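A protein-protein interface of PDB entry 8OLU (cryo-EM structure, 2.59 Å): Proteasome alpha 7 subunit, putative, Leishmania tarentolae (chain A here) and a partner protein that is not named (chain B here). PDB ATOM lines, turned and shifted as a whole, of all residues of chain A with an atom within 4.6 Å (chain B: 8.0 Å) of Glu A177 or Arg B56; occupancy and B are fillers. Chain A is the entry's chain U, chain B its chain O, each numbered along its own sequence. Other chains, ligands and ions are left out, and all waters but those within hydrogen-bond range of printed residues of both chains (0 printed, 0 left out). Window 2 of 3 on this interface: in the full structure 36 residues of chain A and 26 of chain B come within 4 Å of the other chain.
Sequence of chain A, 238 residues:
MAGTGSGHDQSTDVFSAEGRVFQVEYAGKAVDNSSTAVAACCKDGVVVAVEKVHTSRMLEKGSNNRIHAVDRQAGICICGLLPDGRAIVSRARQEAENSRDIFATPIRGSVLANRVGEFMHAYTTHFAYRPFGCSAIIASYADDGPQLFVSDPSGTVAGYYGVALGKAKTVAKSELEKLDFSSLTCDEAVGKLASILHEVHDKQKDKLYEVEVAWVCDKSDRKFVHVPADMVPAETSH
OD1 of Asp B55 is in salt-bridge range of NZ of Lys A173 (3.6 Å).
NH1 of Arg B56 lies within hydrogen-bond range of O of Glu A177, at 2.6 Å.
O of Leu B57 sits at hydrogen-bond distance from N of Tyr A161 (2.7 Å).
OD1 of Asp B55 lies close to N of Leu B57, 3.4 Å away.
Among the printed residues, merely in contact across the chains: Leu A176 with Leu B57 (3.8 Å), Tyr A161 with Arg B59 (3.8 Å), Tyr A161 with Met B58 (3.9 Å) and Glu A177 with Leu B57 (3.97 Å).
Printed residues of chain B within 4 Å of Tyr A161: Leu B57 (2.7 Å), Met B58 (3.9 Å) and Arg B59 (3.8 Å).
Of the printed residues of chain B, Leu A176 touches Leu B57 (3.8 Å).
Glu A177 touches two residues of chain B.
Of the printed residues of chain A, Arg B56 touches Glu A177 (2.6 Å).
Printed residues of chain A within 4 Å of Leu B57: Tyr A161, Leu A176 and Glu A177.
Printed residues of chain A within 4 Å of Met B58: Tyr A161 (3.9 Å).
The nearest residue of chain B that does not touch Glu A177 is Asp B55 (5.3 Å).
The nearest printed residue of chain A that does not touch Leu B57 is Lys A173 (4.3 Å).
Hydrophobic or aromatic side chains of chain B that line the printed part of chain A: Leu B57.
Printed residues of chain A that touch a printed residue of chain B: Tyr A161, Lys A173, Leu A176 and Glu A177.
Hydrophobic or aromatic side chains of chain A that line the printed part of chain B: Tyr A161 and Leu A176.
Along chain A the printed residues that touch a printed residue of chain B span positions 161 to 177.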
ATOM      1  N   TYR A 161     -12.099 -12.401  18.114  1.00  0.00           N
ATOM      2  CA  TYR A 161     -13.500 -12.130  18.380  1.00  0.00           C
ATOM      3  C   TYR A 161     -13.958 -10.952  17.539  1.00  0.00           C
ATOM      4  O   TYR A 161     -15.037 -10.951  16.991  1.00  0.00           O
ATOM      5  CB  TYR A 161     -13.725 -11.815  19.852  1.00  0.00           C
ATOM      6  CG  TYR A 161     -13.411 -12.968  20.759  1.00  0.00           C
ATOM      7  CD1 TYR A 161     -14.028 -14.192  20.571  1.00  0.00           C
ATOM      8  CD2 TYR A 161     -12.475 -12.832  21.778  1.00  0.00           C
ATOM      9  CE1 TYR A 161     -13.696 -15.286  21.369  1.00  0.00           C
ATOM     10  CE2 TYR A 161     -12.125 -13.908  22.580  1.00  0.00           C
ATOM     11  CZ  TYR A 161     -12.757 -15.129  22.391  1.00  0.00           C
ATOM     12  OH  TYR A 161     -12.434 -16.167  23.233  1.00  0.00           O
ATOM     13  N   LYS A 173     -11.187  -0.219  16.187  1.00  0.00           N
ATOM     14  CA  LYS A 173     -10.887  -1.122  17.277  1.00  0.00           C
ATOM     15  C   LYS A 173     -11.387  -0.543  18.605  1.00  0.00           C
ATOM     16  O   LYS A 173     -11.980  -1.256  19.398  1.00  0.00           O
ATOM     17  CB  LYS A 173      -9.384  -1.386  17.279  1.00  0.00           C
ATOM     18  CG  LYS A 173      -8.955  -2.694  17.918  1.00  0.00           C
ATOM     19  CD  LYS A 173      -7.469  -2.713  18.141  1.00  0.00           C
ATOM     20  CE  LYS A 173      -7.043  -3.798  19.101  1.00  0.00           C
ATOM     21  NZ  LYS A 173      -5.978  -3.307  20.010  1.00  0.00           N
ATOM     22  N   SER A 174     -11.193   0.751  18.858  1.00  0.00           N
ATOM     23  CA  SER A 174     -11.728   1.364  20.067  1.00  0.00           C
ATOM     24  C   SER A 174     -13.241   1.170  20.178  1.00  0.00           C
ATOM     25  O   SER A 174     -13.745   1.063  21.292  1.00  0.00           O
ATOM     26  CB  SER A 174     -11.389   2.833  20.149  1.00  0.00           C
ATOM     27  OG  SER A 174     -10.004   3.033  19.921  1.00  0.00           O
ATOM     28  N   GLU A 175     -13.960   1.177  19.048  1.00  0.00           N
ATOM     29  CA  GLU A 175     -15.415   1.061  19.035  1.00  0.00           C
ATOM     30  C   GLU A 175     -15.860  -0.392  19.186  1.00  0.00           C
ATOM     31  O   GLU A 175     -16.948  -0.666  19.684  1.00  0.00           O
ATOM     32  CB  GLU A 175     -16.007   1.551  17.709  1.00  0.00           C
ATOM     33  CG  GLU A 175     -15.988   3.062  17.509  1.00  0.00           C
ATOM     34  CD  GLU A 175     -16.693   3.869  18.594  1.00  0.00           C
ATOM     35  OE1 GLU A 175     -16.038   4.801  19.144  1.00  0.00           O
ATOM     36  OE2 GLU A 175     -17.889   3.559  18.903  1.00  0.00           O
ATOM     37  N   LEU A 176     -15.047  -1.298  18.651  1.00  0.00           N
ATOM     38  CA  LEU A 176     -15.267  -2.720  18.736  1.00  0.00           C
ATOM     39  C   LEU A 176     -14.965  -3.219  20.136  1.00  0.00           C
ATOM     40  O   LEU A 176     -15.325  -4.353  20.444  1.00  0.00           O
ATOM     41  CB  LEU A 176     -14.275  -3.441  17.828  1.00  0.00           C
ATOM     42  CG  LEU A 176     -14.689  -3.779  16.406  1.00  0.00           C
ATOM     43  CD1 LEU A 176     -13.610  -4.655  15.782  1.00  0.00           C
ATOM     44  CD2 LEU A 176     -16.009  -4.496  16.372  1.00  0.00           C
ATOM     45  N   GLU A 177     -14.208  -2.455  20.931  1.00  0.00           N
ATOM     46  CA  GLU A 177     -13.867  -2.913  22.273  1.00  0.00           C
ATOM     47  C   GLU A 177     -15.068  -2.689  23.185  1.00  0.00           C
ATOM     48  O   GLU A 177     -15.312  -3.498  24.081  1.00  0.00           O
ATOM     49  CB  GLU A 177     -12.527  -2.330  22.744  1.00  0.00           C
ATOM     50  CG  GLU A 177     -11.356  -3.164  22.215  1.00  0.00           C
ATOM     51  CD  GLU A 177      -9.924  -2.752  22.553  1.00  0.00           C
ATOM     52  OE1 GLU A 177      -9.331  -3.380  23.473  1.00  0.00           O
ATOM     53  OE2 GLU A 177      -9.370  -1.860  21.856  1.00  0.00           O
ATOM     54  N   LYS A 178     -15.899  -1.704  22.840  1.00  0.00           N
ATOM     55  CA  LYS A 178     -17.110  -1.423  23.592  1.00  0.00           C
ATOM     56  C   LYS A 178     -18.164  -2.528  23.484  1.00  0.00           C
ATOM     57  O   LYS A 178     -19.082  -2.552  24.299  1.00  0.00           O
ATOM     58  CB  LYS A 178     -17.712  -0.090  23.138  1.00  0.00           C
ATOM     59  CG  LYS A 178     -16.769   1.101  23.271  1.00  0.00           C
ATOM     60  CD  LYS A 178     -17.466   2.379  23.686  1.00  0.00           C
ATOM     61  CE  LYS A 178     -16.698   3.640  23.338  1.00  0.00           C
ATOM     62  NZ  LYS A 178     -17.007   4.086  21.959  1.00  0.00           N
ATOM     63  N   LEU A 179     -18.051  -3.435  22.504  1.00  0.00           N
ATOM     64  CA  LEU A 179     -19.009  -4.527  22.340  1.00  0.00           C
ATOM     65  C   LEU A 179     -18.677  -5.699  23.257  1.00  0.00           C
ATOM     66  O   LEU A 179     -17.528  -5.944  23.601  1.00  0.00           O
ATOM     67  CB  LEU A 179     -19.029  -5.006  20.882  1.00  0.00           C
ATOM     68  CG  LEU A 179     -19.248  -3.927  19.813  1.00  0.00           C
ATOM     69  CD1 LEU A 179     -19.373  -4.554  18.422  1.00  0.00           C
ATOM     70  CD2 LEU A 179     -20.472  -3.071  20.132  1.00  0.00           C
ATOM     71  N   ILE B  53      -0.997 -12.161  24.266  1.00  0.00           N
ATOM     72  CA  ILE B  53      -2.208 -11.731  23.601  1.00  0.00           C
ATOM     73  C   ILE B  53      -2.511 -10.350  24.159  1.00  0.00           C
ATOM     74  O   ILE B  53      -3.296 -10.196  25.089  1.00  0.00           O
ATOM     75  CB  ILE B  53      -3.352 -12.743  23.834  1.00  0.00           C
ATOM     76  CG1 ILE B  53      -2.880 -14.193  23.688  1.00  0.00           C
ATOM     77  CG2 ILE B  53      -4.537 -12.476  22.913  1.00  0.00           C
ATOM     78  CD1 ILE B  53      -2.494 -14.568  22.265  1.00  0.00           C
ATOM     79  N   PRO B  54      -1.841  -9.304  23.643  1.00  0.00           N
ATOM     80  CA  PRO B  54      -2.085  -7.952  24.142  1.00  0.00           C
ATOM     81  C   PRO B  54      -3.491  -7.486  23.736  1.00  0.00           C
ATOM     82  O   PRO B  54      -4.226  -6.929  24.555  1.00  0.00           O
ATOM     83  CB  PRO B  54      -0.917  -7.154  23.522  1.00  0.00           C
ATOM     84  CG  PRO B  54      -0.482  -7.931  22.272  1.00  0.00           C
ATOM     85  CD  PRO B  54      -0.865  -9.368  22.536  1.00  0.00           C
ATOM     86  N   ASP B  55      -3.853  -7.782  22.469  1.00  0.00           N
ATOM     87  CA  ASP B  55      -5.135  -7.470  21.845  1.00  0.00           C
ATOM     88  C   ASP B  55      -6.247  -8.217  22.585  1.00  0.00           C
ATOM     89  O   ASP B  55      -6.278  -9.440  22.572  1.00  0.00           O
ATOM     90  CB  ASP B  55      -5.042  -7.812  20.348  1.00  0.00           C
ATOM     91  CG  ASP B  55      -6.139  -7.282  19.421  1.00  0.00           C
ATOM     92  OD1 ASP B  55      -7.137  -6.708  19.921  1.00  0.00           O
ATOM     93  OD2 ASP B  55      -5.979  -7.437  18.187  1.00  0.00           O
ATOM     94  N   ARG B  56      -7.152  -7.472  23.233  1.00  0.00           N
ATOM     95  CA  ARG B  56      -8.139  -8.053  24.132  1.00  0.00           C
ATOM     96  C   ARG B  56      -9.131  -8.859  23.294  1.00  0.00           C
ATOM     97  O   ARG B  56      -9.731  -9.825  23.764  1.00  0.00           O
ATOM     98  CB  ARG B  56      -8.763  -6.926  24.973  1.00  0.00           C
ATOM     99  CG  ARG B  56      -9.561  -7.379  26.196  1.00  0.00           C
ATOM    100  CD  ARG B  56     -11.073  -7.488  25.990  1.00  0.00           C
ATOM    101  NE  ARG B  56     -11.722  -6.178  25.884  1.00  0.00           N
ATOM    102  CZ  ARG B  56     -12.960  -5.954  25.436  1.00  0.00           C
ATOM    103  NH1 ARG B  56     -13.373  -4.713  25.243  1.00  0.00           N
ATOM    104  NH2 ARG B  56     -13.771  -6.963  25.156  1.00  0.00           N
ATOM    105  N   LEU B  57      -9.195  -8.465  22.011  1.00  0.00           N
ATOM    106  CA  LEU B  57     -10.161  -8.908  21.024  1.00  0.00           C
ATOM    107  C   LEU B  57      -9.673 -10.097  20.220  1.00  0.00           C
ATOM    108  O   LEU B  57     -10.440 -10.667  19.443  1.00  0.00           O
ATOM    109  CB  LEU B  57     -10.351  -7.776  20.025  1.00  0.00           C
ATOM    110  CG  LEU B  57     -11.349  -6.682  20.385  1.00  0.00           C
ATOM    111  CD1 LEU B  57     -11.667  -5.834  19.147  1.00  0.00           C
ATOM    112  CD2 LEU B  57     -12.608  -7.279  20.968  1.00  0.00           C
ATOM    113  N   MET B  58      -8.379 -10.396  20.315  1.00  0.00           N
ATOM    114  CA  MET B  58      -7.828 -11.595  19.728  1.00  0.00           C
ATOM    115  C   MET B  58      -8.224 -12.792  20.582  1.00  0.00           C
ATOM    116  O   MET B  58      -8.489 -12.664  21.777  1.00  0.00           O
ATOM    117  CB  MET B  58      -6.317 -11.474  19.634  1.00  0.00           C
ATOM    118  CG  MET B  58      -5.669 -12.509  18.718  1.00  0.00           C
ATOM    119  SD  MET B  58      -3.880 -12.287  18.480  1.00  0.00           S
ATOM    120  CE  MET B  58      -3.785 -10.908  17.335  1.00  0.00           C
ATOM    121  N   ARG B  59      -8.331 -13.942  19.919  1.00  0.00           N
ATOM    122  CA  ARG B  59      -8.919 -15.140  20.473  1.00  0.00           C
ATOM    123  C   ARG B  59      -7.772 -16.016  20.935  1.00  0.00           C
ATOM    124  O   ARG B  59      -7.113 -16.638  20.124  1.00  0.00           O
ATOM    125  CB  ARG B  59      -9.778 -15.826  19.409  1.00  0.00           C
ATOM    126  CG  ARG B  59     -10.493 -17.100  19.830  1.00  0.00           C
ATOM    127  CD  ARG B  59     -11.655 -17.382  18.907  1.00  0.00           C
ATOM    128  NE  ARG B  59     -12.514 -18.504  19.306  1.00  0.00           N
ATOM    129  CZ  ARG B  59     -13.672 -18.847  18.703  1.00  0.00           C
ATOM    130  NH1 ARG B  59     -14.269 -19.993  18.985  1.00  0.00           N
ATOM    131  NH2 ARG B  59     -14.230 -18.056  17.797  1.00  0.00           N
ATOM    132  N   PRO B  60      -7.439 -16.069  22.232  1.00  0.00           N
ATOM    133  CA  PRO B  60      -6.175 -16.685  22.636  1.00  0.00           C
ATOM    134  C   PRO B  60      -5.943 -18.092  22.091  1.00  0.00           C
ATOM    135  O   PRO B  60      -4.824 -18.388  21.697  1.00  0.00           O
ATOM    136  CB  PRO B  60      -6.232 -16.603  24.168  1.00  0.00           C
ATOM    137  CG  PRO B  60      -7.721 -16.441  24.452  1.00  0.00           C
ATOM    138  CD  PRO B  60      -8.203 -15.517  23.360  1.00  0.00           C
